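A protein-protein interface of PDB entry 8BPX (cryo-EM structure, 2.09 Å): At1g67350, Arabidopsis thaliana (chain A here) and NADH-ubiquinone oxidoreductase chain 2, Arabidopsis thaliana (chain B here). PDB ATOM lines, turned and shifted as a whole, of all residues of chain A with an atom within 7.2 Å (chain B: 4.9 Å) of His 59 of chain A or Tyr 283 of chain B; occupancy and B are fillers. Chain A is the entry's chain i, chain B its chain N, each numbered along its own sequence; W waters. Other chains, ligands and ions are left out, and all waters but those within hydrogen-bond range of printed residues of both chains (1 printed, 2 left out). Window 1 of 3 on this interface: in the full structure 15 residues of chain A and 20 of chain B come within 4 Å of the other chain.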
ATOM      1  N   PRO A  50     -19.142  -1.857 -10.060  1.00  0.00           N
ATOM      2  CA  PRO A  50     -19.003  -0.749 -10.987  1.00  0.00           C
ATOM      3  C   PRO A  50     -19.054  -1.196 -12.456  1.00  0.00           C
ATOM      4  O   PRO A  50     -18.941  -2.368 -12.712  1.00  0.00           O
ATOM      5  CB  PRO A  50     -17.659  -0.143 -10.520  1.00  0.00           C
ATOM      6  CG  PRO A  50     -16.878  -1.267  -9.960  1.00  0.00           C
ATOM      7  CD  PRO A  50     -17.938  -2.024  -9.217  1.00  0.00           C
ATOM      8  N   GLY A  52     -17.739  -2.207 -15.734  1.00  0.00           N
ATOM      9  CA  GLY A  52     -16.483  -2.702 -16.261  1.00  0.00           C
ATOM     10  C   GLY A  52     -15.355  -2.715 -15.250  1.00  0.00           C
ATOM     11  O   GLY A  52     -14.266  -2.215 -15.534  1.00  0.00           O
ATOM     12  N   PHE A  53     -15.605  -3.267 -14.060  1.00  0.00           N
ATOM     13  CA  PHE A  53     -14.569  -3.274 -13.032  1.00  0.00           C
ATOM     14  C   PHE A  53     -13.349  -4.067 -13.485  1.00  0.00           C
ATOM     15  O   PHE A  53     -12.211  -3.687 -13.194  1.00  0.00           O
ATOM     16  CB  PHE A  53     -15.121  -3.833 -11.721  1.00  0.00           C
ATOM     17  CG  PHE A  53     -15.601  -5.252 -11.815  1.00  0.00           C
ATOM     18  CD1 PHE A  53     -16.885  -5.538 -12.244  1.00  0.00           C
ATOM     19  CD2 PHE A  53     -14.770  -6.302 -11.467  1.00  0.00           C
ATOM     20  CE1 PHE A  53     -17.324  -6.846 -12.327  1.00  0.00           C
ATOM     21  CE2 PHE A  53     -15.207  -7.608 -11.551  1.00  0.00           C
ATOM     22  CZ  PHE A  53     -16.482  -7.880 -11.979  1.00  0.00           C
ATOM     23  N   TRP A  54     -13.565  -5.157 -14.225  1.00  0.00           N
ATOM     24  CA  TRP A  54     -12.465  -5.976 -14.722  1.00  0.00           C
ATOM     25  C   TRP A  54     -11.567  -5.226 -15.698  1.00  0.00           C
ATOM     26  O   TRP A  54     -10.472  -5.710 -16.000  1.00  0.00           O
ATOM     27  CB  TRP A  54     -13.019  -7.243 -15.377  1.00  0.00           C
ATOM     28  CG  TRP A  54     -13.899  -6.942 -16.538  1.00  0.00           C
ATOM     29  CD1 TRP A  54     -13.516  -6.779 -17.828  1.00  0.00           C
ATOM     30  CD2 TRP A  54     -15.316  -6.734 -16.509  1.00  0.00           C
ATOM     31  NE1 TRP A  54     -14.604  -6.490 -18.615  1.00  0.00           N
ATOM     32  CE2 TRP A  54     -15.724  -6.457 -17.828  1.00  0.00           C
ATOM     33  CE3 TRP A  54     -16.278  -6.759 -15.499  1.00  0.00           C
ATOM     34  CZ2 TRP A  54     -17.052  -6.212 -18.161  1.00  0.00           C
ATOM     35  CZ3 TRP A  54     -17.597  -6.513 -15.831  1.00  0.00           C
ATOM     36  CH2 TRP A  54     -17.972  -6.243 -17.151  1.00  0.00           C
ATOM     37  N   THR A  55     -12.007  -4.072 -16.204  1.00  0.00           N
ATOM     38  CA  THR A  55     -11.149  -3.193 -16.990  1.00  0.00           C
ATOM     39  C   THR A  55     -10.098  -2.485 -16.142  1.00  0.00           C
ATOM     40  O   THR A  55      -9.036  -2.128 -16.666  1.00  0.00           O
ATOM     41  CB  THR A  55     -12.015  -2.162 -17.727  1.00  0.00           C
ATOM     42  OG1 THR A  55     -12.996  -2.842 -18.517  1.00  0.00           O
ATOM     43  CG2 THR A  55     -11.181  -1.262 -18.626  1.00  0.00           C
ATOM     44  N   PHE A  56     -10.365  -2.270 -14.840  1.00  0.00           N
ATOM     45  CA  PHE A  56      -9.479  -1.519 -13.931  1.00  0.00           C
ATOM     46  C   PHE A  56      -8.099  -2.211 -13.842  1.00  0.00           C
ATOM     47  O   PHE A  56      -8.065  -3.447 -13.706  1.00  0.00           O
ATOM     48  CB  PHE A  56     -10.182  -1.296 -12.600  1.00  0.00           C
ATOM     49  CG  PHE A  56     -11.552  -0.670 -12.597  1.00  0.00           C
ATOM     50  CD1 PHE A  56     -12.008   0.095 -13.655  1.00  0.00           C
ATOM     51  CD2 PHE A  56     -12.395  -0.858 -11.515  1.00  0.00           C
ATOM     52  CE1 PHE A  56     -13.277   0.648 -13.637  1.00  0.00           C
ATOM     53  CE2 PHE A  56     -13.672  -0.316 -11.502  1.00  0.00           C
ATOM     54  CZ  PHE A  56     -14.104   0.440 -12.562  1.00  0.00           C
ATOM     55  N   GLU A  57      -7.015  -1.450 -13.916  1.00  0.00           N
ATOM     56  CA  GLU A  57      -5.661  -1.971 -14.078  1.00  0.00           C
ATOM     57  C   GLU A  57      -5.313  -3.017 -13.027  1.00  0.00           C
ATOM     58  O   GLU A  57      -4.575  -3.964 -13.320  1.00  0.00           O
ATOM     59  CB  GLU A  57      -4.650  -0.824 -14.034  1.00  0.00           C
ATOM     60  CG  GLU A  57      -4.540  -0.048 -15.336  1.00  0.00           C
ATOM     61  CD  GLU A  57      -5.728   0.866 -15.576  1.00  0.00           C
ATOM     62  OE1 GLU A  57      -6.463   1.157 -14.608  1.00  0.00           O
ATOM     63  OE2 GLU A  57      -5.927   1.294 -16.732  1.00  0.00           O
ATOM     64  N   ARG A  58      -5.827  -2.865 -11.802  1.00  0.00           N
ATOM     65  CA  ARG A  58      -5.565  -3.854 -10.762  1.00  0.00           C
ATOM     66  C   ARG A  58      -6.009  -5.250 -11.190  1.00  0.00           C
ATOM     67  O   ARG A  58      -5.421  -6.248 -10.760  1.00  0.00           O
ATOM     68  CB  ARG A  58      -6.264  -3.445  -9.463  1.00  0.00           C
ATOM     69  CG  ARG A  58      -6.300  -4.522  -8.387  1.00  0.00           C
ATOM     70  CD  ARG A  58      -4.915  -4.779  -7.813  1.00  0.00           C
ATOM     71  NE  ARG A  58      -4.187  -5.814  -8.538  1.00  0.00           N
ATOM     72  CZ  ARG A  58      -2.908  -6.106  -8.341  1.00  0.00           C
ATOM     73  NH1 ARG A  58      -2.184  -5.467  -7.438  1.00  0.00           N
ATOM     74  NH2 ARG A  58      -2.342  -7.067  -9.066  1.00  0.00           N
ATOM     75  N   HIS A  59      -6.990  -5.315 -12.076  1.00  0.00           N
ATOM     76  CA  HIS A  59      -7.550  -6.621 -12.458  1.00  0.00           C
ATOM     77  C   HIS A  59      -6.890  -7.206 -13.725  1.00  0.00           C
ATOM     78  O   HIS A  59      -7.231  -8.297 -14.116  1.00  0.00           O
ATOM     79  CB  HIS A  59      -9.029  -6.416 -12.572  1.00  0.00           C
ATOM     80  CG  HIS A  59      -9.714  -5.763 -11.411  1.00  0.00           C
ATOM     81  ND1 HIS A  59     -11.069  -5.558 -11.396  1.00  0.00           N
ATOM     82  CD2 HIS A  59      -9.252  -5.253 -10.250  1.00  0.00           C
ATOM     83  CE1 HIS A  59     -11.416  -4.953 -10.282  1.00  0.00           C
ATOM     84  NE2 HIS A  59     -10.319  -4.749  -9.564  1.00  0.00           N
ATOM     85  N   ASN A  60      -6.023  -6.455 -14.358  1.00  0.00           N
ATOM     86  CA  ASN A  60      -5.356  -6.904 -15.575  1.00  0.00           C
ATOM     87  C   ASN A  60      -3.916  -7.320 -15.293  1.00  0.00           C
ATOM     88  O   ASN A  60      -3.019  -7.105 -16.110  1.00  0.00           O
ATOM     89  CB  ASN A  60      -5.400  -5.821 -16.649  1.00  0.00           C
ATOM     90  CG  ASN A  60      -6.797  -5.603 -17.203  1.00  0.00           C
ATOM     91  OD1 ASN A  60      -7.649  -6.490 -17.144  1.00  0.00           O
ATOM     92  ND2 ASN A  60      -7.037  -4.413 -17.747  1.00  0.00           N
ATOM     93  N   ALA A  61      -3.683  -7.918 -14.124  1.00  0.00           N
ATOM     94  CA  ALA A  61      -2.323  -8.274 -13.733  1.00  0.00           C
ATOM     95  C   ALA A  61      -1.706  -9.283 -14.697  1.00  0.00           C
ATOM     96  O   ALA A  61      -0.538  -9.149 -15.073  1.00  0.00           O
ATOM     97  CB  ALA A  61      -2.316  -8.819 -12.304  1.00  0.00           C
ATOM     98  N   GLN A  62      -2.474 -10.294 -15.113  1.00  0.00           N
ATOM     99  CA  GLN A  62      -1.909 -11.334 -15.968  1.00  0.00           C
ATOM    100  C   GLN A  62      -1.539 -10.785 -17.345  1.00  0.00           C
ATOM    101  O   GLN A  62      -0.535 -11.199 -17.931  1.00  0.00           O
ATOM    102  CB  GLN A  62      -2.879 -12.514 -16.086  1.00  0.00           C
ATOM    103  CG  GLN A  62      -2.527 -13.511 -17.189  1.00  0.00           C
ATOM    104  CD  GLN A  62      -3.406 -14.756 -17.186  1.00  0.00           C
ATOM    105  OE1 GLN A  62      -4.601 -14.690 -16.905  1.00  0.00           O
ATOM    106  NE2 GLN A  62      -2.811 -15.897 -17.509  1.00  0.00           N
ATOM    107  N   LEU A  63      -2.330  -9.843 -17.867  1.00  0.00           N
ATOM    108  CA  LEU A  63      -2.022  -9.239 -19.160  1.00  0.00           C
ATOM    109  C   LEU A  63      -0.673  -8.533 -19.171  1.00  0.00           C
ATOM    110  O   LEU A  63      -0.083  -8.373 -20.243  1.00  0.00           O
ATOM    111  CB  LEU A  63      -3.118  -8.250 -19.556  1.00  0.00           C
ATOM    112  CG  LEU A  63      -4.442  -8.820 -20.074  1.00  0.00           C
ATOM    113  CD1 LEU A  63      -5.166  -7.782 -20.898  1.00  0.00           C
ATOM    114  CD2 LEU A  63      -4.222 -10.080 -20.887  1.00  0.00           C
ATOM    115  N   ARG A  64      -0.170  -8.105 -18.014  1.00  0.00           N
ATOM    116  CA  ARG A  64       1.118  -7.429 -17.946  1.00  0.00           C
ATOM    117  C   ARG A  64       2.244  -8.317 -17.439  1.00  0.00           C
ATOM    118  O   ARG A  64       3.408  -8.050 -17.752  1.00  0.00           O
ATOM    119  CB  ARG A  64       1.021  -6.189 -17.053  1.00  0.00           C
ATOM    120  CG  ARG A  64      -0.261  -5.407 -17.237  1.00  0.00           C
ATOM    121  CD  ARG A  64      -0.036  -3.926 -16.997  1.00  0.00           C
ATOM    122  NE  ARG A  64       0.297  -3.635 -15.607  1.00  0.00           N
ATOM    123  CZ  ARG A  64      -0.552  -3.732 -14.593  1.00  0.00           C
ATOM    124  NH1 ARG A  64      -1.804  -4.122 -14.771  1.00  0.00           N
ATOM    125  NH2 ARG A  64      -0.135  -3.428 -13.368  1.00  0.00           N
ATOM    126  N   ARG B  88      -2.685 -11.413  -3.225  1.00  0.00           N
ATOM    127  CA  ARG B  88      -3.020 -10.046  -3.616  1.00  0.00           C
ATOM    128  C   ARG B  88      -3.249  -9.212  -2.367  1.00  0.00           C
ATOM    129  O   ARG B  88      -4.187  -9.477  -1.610  1.00  0.00           O
ATOM    130  CB  ARG B  88      -4.265 -10.008  -4.508  1.00  0.00           C
ATOM    131  CG  ARG B  88      -4.552  -8.632  -5.089  1.00  0.00           C
ATOM    132  CD  ARG B  88      -5.511  -8.709  -6.259  1.00  0.00           C
ATOM    133  NE  ARG B  88      -4.832  -9.073  -7.497  1.00  0.00           N
ATOM    134  CZ  ARG B  88      -5.370  -8.965  -8.702  1.00  0.00           C
ATOM    135  NH1 ARG B  88      -6.589  -8.479  -8.872  1.00  0.00           N
ATOM    136  NH2 ARG B  88      -4.672  -9.362  -9.762  1.00  0.00           N
ATOM    137  N   TYR B 143      -5.738 -15.108  -3.255  1.00  0.00           N
ATOM    138  CA  TYR B 143      -6.410 -14.651  -4.464  1.00  0.00           C
ATOM    139  C   TYR B 143      -6.508 -15.773  -5.495  1.00  0.00           C
ATOM    140  O   TYR B 143      -6.579 -15.516  -6.701  1.00  0.00           O
ATOM    141  CB  TYR B 143      -5.698 -13.430  -5.047  1.00  0.00           C
ATOM    142  CG  TYR B 143      -6.624 -12.490  -5.775  1.00  0.00           C
ATOM    143  CD1 TYR B 143      -7.670 -11.854  -5.117  1.00  0.00           C
ATOM    144  CD2 TYR B 143      -6.457 -12.245  -7.126  1.00  0.00           C
ATOM    145  CE1 TYR B 143      -8.524 -11.000  -5.794  1.00  0.00           C
ATOM    146  CE2 TYR B 143      -7.298 -11.405  -7.809  1.00  0.00           C
ATOM    147  CZ  TYR B 143      -8.326 -10.780  -7.143  1.00  0.00           C
ATOM    148  OH  TYR B 143      -9.149  -9.943  -7.848  1.00  0.00           O
ATOM    149  N   ASP B 207      -8.951 -13.431 -10.521  1.00  0.00           N
ATOM    150  CA  ASP B 207      -9.146 -12.524 -11.652  1.00  0.00           C
ATOM    151  C   ASP B 207      -9.693 -13.266 -12.864  1.00  0.00           C
ATOM    152  O   ASP B 207     -10.648 -12.814 -13.514  1.00  0.00           O
ATOM    153  CB  ASP B 207      -7.827 -11.842 -12.012  1.00  0.00           C
ATOM    154  CG  ASP B 207      -7.620 -10.546 -11.275  1.00  0.00           C
ATOM    155  OD1 ASP B 207      -6.469 -10.070 -11.239  1.00  0.00           O
ATOM    156  OD2 ASP B 207      -8.600 -10.008 -10.724  1.00  0.00           O
ATOM    157  N   ALA B 210     -13.252 -14.186 -12.309  1.00  0.00           N
ATOM    158  CA  ALA B 210     -14.107 -13.019 -12.483  1.00  0.00           C
ATOM    159  C   ALA B 210     -14.369 -12.755 -13.961  1.00  0.00           C
ATOM    160  O   ALA B 210     -15.514 -12.547 -14.371  1.00  0.00           O
ATOM    161  CB  ALA B 210     -13.475 -11.797 -11.812  1.00  0.00           C
ATOM    162  N   LYS B 211     -13.319 -12.791 -14.786  1.00  0.00           N
ATOM    163  CA  LYS B 211     -13.506 -12.519 -16.210  1.00  0.00           C
ATOM    164  C   LYS B 211     -14.409 -13.557 -16.871  1.00  0.00           C
ATOM    165  O   LYS B 211     -15.306 -13.203 -17.644  1.00  0.00           O
ATOM    166  CB  LYS B 211     -12.157 -12.453 -16.923  1.00  0.00           C
ATOM    167  CG  LYS B 211     -11.464 -11.110 -16.803  1.00  0.00           C
ATOM    168  CD  LYS B 211     -10.011 -11.200 -17.227  1.00  0.00           C
ATOM    169  CE  LYS B 211      -9.408  -9.824 -17.434  1.00  0.00           C
ATOM    170  NZ  LYS B 211      -9.360  -9.051 -16.167  1.00  0.00           N
ATOM    171  N   LEU B 278     -15.926 -12.565   0.963  1.00  0.00           N
ATOM    172  CA  LEU B 278     -16.041 -11.329   0.201  1.00  0.00           C
ATOM    173  C   LEU B 278     -15.263 -11.431  -1.103  1.00  0.00           C
ATOM    174  O   LEU B 278     -15.840 -11.310  -2.190  1.00  0.00           O
ATOM    175  CB  LEU B 278     -15.551 -10.146   1.043  1.00  0.00           C
ATOM    176  CG  LEU B 278     -16.376  -9.761   2.280  1.00  0.00           C
ATOM    177  CD1 LEU B 278     -16.133  -8.322   2.698  1.00  0.00           C
ATOM    178  CD2 LEU B 278     -17.854  -9.992   2.047  1.00  0.00           C
ATOM    179  N   ARG B 279     -13.974 -11.784  -1.012  1.00  0.00           N
ATOM    180  CA  ARG B 279     -13.118 -11.773  -2.195  1.00  0.00           C
ATOM    181  C   ARG B 279     -13.437 -12.885  -3.185  1.00  0.00           C
ATOM    182  O   ARG B 279     -13.083 -12.765  -4.361  1.00  0.00           O
ATOM    183  CB  ARG B 279     -11.650 -11.866  -1.792  1.00  0.00           C
ATOM    184  CG  ARG B 279     -11.142 -10.665  -1.036  1.00  0.00           C
ATOM    185  CD  ARG B 279      -9.652 -10.774  -0.807  1.00  0.00           C
ATOM    186  NE  ARG B 279      -8.919  -9.755  -1.545  1.00  0.00           N
ATOM    187  CZ  ARG B 279      -7.630  -9.835  -1.841  1.00  0.00           C
ATOM    188  NH1 ARG B 279      -6.907 -10.888  -1.495  1.00  0.00           N
ATOM    189  NH2 ARG B 279      -7.053  -8.836  -2.502  1.00  0.00           N
ATOM    190  N   VAL B 280     -14.062 -13.971  -2.750  1.00  0.00           N
ATOM    191  CA  VAL B 280     -14.450 -15.021  -3.684  1.00  0.00           C
ATOM    192  C   VAL B 280     -15.767 -14.682  -4.361  1.00  0.00           C
ATOM    193  O   VAL B 280     -15.831 -14.506  -5.581  1.00  0.00           O
ATOM    194  CB  VAL B 280     -14.532 -16.383  -2.961  1.00  0.00           C
ATOM    195  CG1 VAL B 280     -15.244 -17.397  -3.827  1.00  0.00           C
ATOM    196  CG2 VAL B 280     -13.158 -16.884  -2.588  1.00  0.00           C
ATOM    197  N   PHE B 281     -16.826 -14.527  -3.570  1.00  0.00           N
ATOM    198  CA  PHE B 281     -18.164 -14.392  -4.119  1.00  0.00           C
ATOM    199  C   PHE B 281     -18.451 -12.993  -4.645  1.00  0.00           C
ATOM    200  O   PHE B 281     -18.870 -12.840  -5.796  1.00  0.00           O
ATOM    201  CB  PHE B 281     -19.195 -14.787  -3.062  1.00  0.00           C
ATOM    202  CG  PHE B 281     -19.037 -16.194  -2.559  1.00  0.00           C
ATOM    203  CD1 PHE B 281     -18.569 -17.191  -3.398  1.00  0.00           C
ATOM    204  CD2 PHE B 281     -19.413 -16.534  -1.273  1.00  0.00           C
ATOM    205  CE1 PHE B 281     -18.441 -18.491  -2.958  1.00  0.00           C
ATOM    206  CE2 PHE B 281     -19.292 -17.833  -0.826  1.00  0.00           C
ATOM    207  CZ  PHE B 281     -18.806 -18.815  -1.675  1.00  0.00           C
ATOM    208  N   ILE B 282     -18.502 -12.028  -3.736  1.00  0.00           N
ATOM    209  CA  ILE B 282     -18.619 -10.583  -4.083  1.00  0.00           C
ATOM    210  C   ILE B 282     -17.751 -10.170  -5.291  1.00  0.00           C
ATOM    211  O   ILE B 282     -18.332  -9.493  -6.169  1.00  0.00           O
ATOM    212  CB  ILE B 282     -18.285  -9.793  -2.777  1.00  0.00           C
ATOM    213  CG1 ILE B 282     -19.474  -9.653  -1.825  1.00  0.00           C
ATOM    214  CG2 ILE B 282     -17.612  -8.466  -3.082  1.00  0.00           C
ATOM    215  CD1 ILE B 282     -20.422  -8.548  -2.199  1.00  0.00           C
ATOM    216  N   TYR B 283     -16.498 -10.635  -5.442  1.00  0.00           N
ATOM    217  CA  TYR B 283     -15.542 -10.286  -6.476  1.00  0.00           C
ATOM    218  C   TYR B 283     -15.689 -11.182  -7.702  1.00  0.00           C
ATOM    219  O   TYR B 283     -15.256 -10.795  -8.794  1.00  0.00           O
ATOM    220  CB  TYR B 283     -14.144 -10.389  -5.867  1.00  0.00           C
ATOM    221  CG  TYR B 283     -13.090  -9.453  -6.396  1.00  0.00           C
ATOM    222  CD1 TYR B 283     -13.266  -8.733  -7.568  1.00  0.00           C
ATOM    223  CD2 TYR B 283     -11.932  -9.242  -5.660  1.00  0.00           C
ATOM    224  CE1 TYR B 283     -12.287  -7.858  -8.012  1.00  0.00           C
ATOM    225  CE2 TYR B 283     -10.963  -8.376  -6.083  1.00  0.00           C
ATOM    226  CZ  TYR B 283     -11.136  -7.688  -7.257  1.00  0.00           C
ATOM    227  OH  TYR B 283     -10.142  -6.829  -7.658  1.00  0.00           O
ATOM    228  N   GLY B 284     -16.442 -12.268  -7.523  1.00  0.00           N
ATOM    229  CA  GLY B 284     -16.663 -13.280  -8.580  1.00  0.00           C
ATOM    230  C   GLY B 284     -18.045 -13.167  -9.176  1.00  0.00           C
ATOM    231  O   GLY B 284     -18.618 -12.081  -9.048  1.00  0.00           O
ATOM    232  N   SER B 285     -18.576 -14.252  -9.754  1.00  0.00           N
ATOM    233  CA  SER B 285     -19.902 -14.078 -10.395  1.00  0.00           C
ATOM    234  C   SER B 285     -20.729 -15.299 -10.709  1.00  0.00           C
ATOM    235  O   SER B 285     -20.559 -15.800 -11.804  1.00  0.00           O
ATOM    236  CB  SER B 285     -19.780 -13.294 -11.642  1.00  0.00           C
ATOM    237  OG  SER B 285     -19.818 -11.898 -11.367  1.00  0.00           O
ATOM    238  N   LEU B 497     -12.743  -3.490  -2.440  1.00  0.00           N
ATOM    239  CA  LEU B 497     -13.039  -4.824  -3.031  1.00  0.00           C
ATOM    240  C   LEU B 497     -13.158  -4.716  -4.564  1.00  0.00           C
ATOM    241  O   LEU B 497     -12.642  -5.562  -5.218  1.00  0.00           O
ATOM    242  CB  LEU B 497     -14.348  -5.311  -2.416  1.00  0.00           C
ATOM    243  CG  LEU B 497     -14.250  -5.949  -1.032  1.00  0.00           C
ATOM    244  CD1 LEU B 497     -15.624  -6.339  -0.513  1.00  0.00           C
ATOM    245  CD2 LEU B 497     -13.312  -7.144  -1.032  1.00  0.00           C
ATOM    246  N   TYR B 498     -13.643  -3.605  -5.092  1.00  0.00           N
ATOM    247  CA  TYR B 498     -13.859  -3.446  -6.568  1.00  0.00           C
ATOM    248  C   TYR B 498     -13.094  -2.274  -7.146  1.00  0.00           C
ATOM    249  O   TYR B 498     -13.322  -1.977  -8.268  1.00  0.00           O
ATOM    250  CB  TYR B 498     -15.313  -3.085  -6.795  1.00  0.00           C
ATOM    251  CG  TYR B 498     -16.264  -3.774  -5.863  1.00  0.00           C
ATOM    252  CD1 TYR B 498     -16.607  -3.202  -4.653  1.00  0.00           C
ATOM    253  CD2 TYR B 498     -16.772  -5.024  -6.169  1.00  0.00           C
ATOM    254  CE1 TYR B 498     -17.450  -3.852  -3.771  1.00  0.00           C
ATOM    255  CE2 TYR B 498     -17.625  -5.678  -5.305  1.00  0.00           C
ATOM    256  CZ  TYR B 498     -17.956  -5.092  -4.100  1.00  0.00           C
ATOM    257  OH  TYR B 498     -18.790  -5.721  -3.228  1.00  0.00           O
HETATM  258  O   HOH W   1      -4.920 -10.763 -13.831  1.00  0.00           O
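NH1 of Arg 88 of chain B is in hydrogen-bond range of O of Arg 58 of chain A.
O of His 59 of chain A sits at hydrogen-bond distance from NZ of Lys 211 of chain B.
The side-chain amino group (NZ) of Lys 211 of chain B is in hydrogen-bond range of the side-chain amide oxygen (OD1) of Asn 60 of chain A (3.2 Å).
The side-chain hydroxyl (OH) of Tyr 283 of chain B lies within hydrogen-bond range of a ring nitrogen (NE2) of His 59 of chain A (2.8 Å).
O of His 59 of chain A lies close to OD1 of Asp 207 of chain B (3.5 Å).
NH1 of Arg 88 of chain B is in hydrogen-bond range of OH of Tyr 143 of chain B (3.1 Å).
The side-chain hydroxyl (OH) of Tyr 143 of chain B lies close to the side-chain hydroxyl (OH) of Tyr 283 of chain B (3.3 Å).
O of Phe 53 of chain A sits at hydrogen-bond distance from ND1 of His 59 of chain A.
The backbone carbonyl oxygen of Trp 54 of chain A sits close to the side-chain amide oxygen of Asn 60 of chain A (3.1 Å).
O of Thr 55 of chain A sits at hydrogen-bond distance from ND2 of Asn 60 of chain A.
O of Asn 60 of chain A sits close to NH1 of Arg 64 of chain A, 3.5 Å away.
Pro 50 of chain A touches Tyr 498 of chain B (CD to CB, 3.7 Å).
NZ of Lys 211 of chain B touches O of Trp 54 of chain A, at 3.5 Å.
CD2 of Phe 56 of chain A touches O of Tyr 498 of chain B, at 3.6 Å.
Arg 58 of chain A touches Asp 207 of chain B.
Ala 61 of chain A touches Arg 88 of chain B (CB to NH2, 3.5 Å).
Of the printed residues of chain B, His 59 of chain A touches Asp 207 (3.5 Å), Lys 211 (3.1 Å) and Tyr 283 (2.8 Å).
Printed residues of chain B within 4 Å of Asn 60 of chain A: Lys 211 (3.2 Å).
Of the printed residues of chain B, Ala 61 of chain A touches Arg 88.
Of the printed residues of chain A, Arg 88 of chain B touches Arg 58 and Ala 61.
Printed residues of chain A within 4 Å of Asp 207 of chain B: Arg 58 (3.99 Å) and His 59 (3.5 Å).
Tyr 283 of chain B touches just one residue of chain A: His 59.
Printed residues of chain A within 4 Å of Tyr 498 of chain B: Pro 50 and Phe 56.
The nearest residue of chain A that does not touch Tyr 283 of chain B is Phe 53 of chain A (4.2 Å).
The nearest printed residue of chain B that does not touch Ala 61 of chain A is Asp 207 of chain B (4.5 Å).
Printed residues of chain A that touch a printed residue of chain B: Pro 50, Trp 54, Phe 56, Arg 58, His 59, Asn 60 and Ala 61.
Along chain A the printed residues that touch a printed residue of chain B span positions 50 to 61.
Printed residues of chain B that touch a printed residue of chain A: Arg 88, Asp 207, Lys 211, Tyr 283 and Tyr 498.
Water W1 lies within hydrogen-bond range of the backbone NH of Gln 62 of chain A (2.8 Å), the side-chain carboxylate of Asp 207 of chain B (3.1 Å), the backbone NH of Ala 61 of chain A (3.1 Å) and the backbone carbonyl oxygen of His 59 of chain A (3.4 Å).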
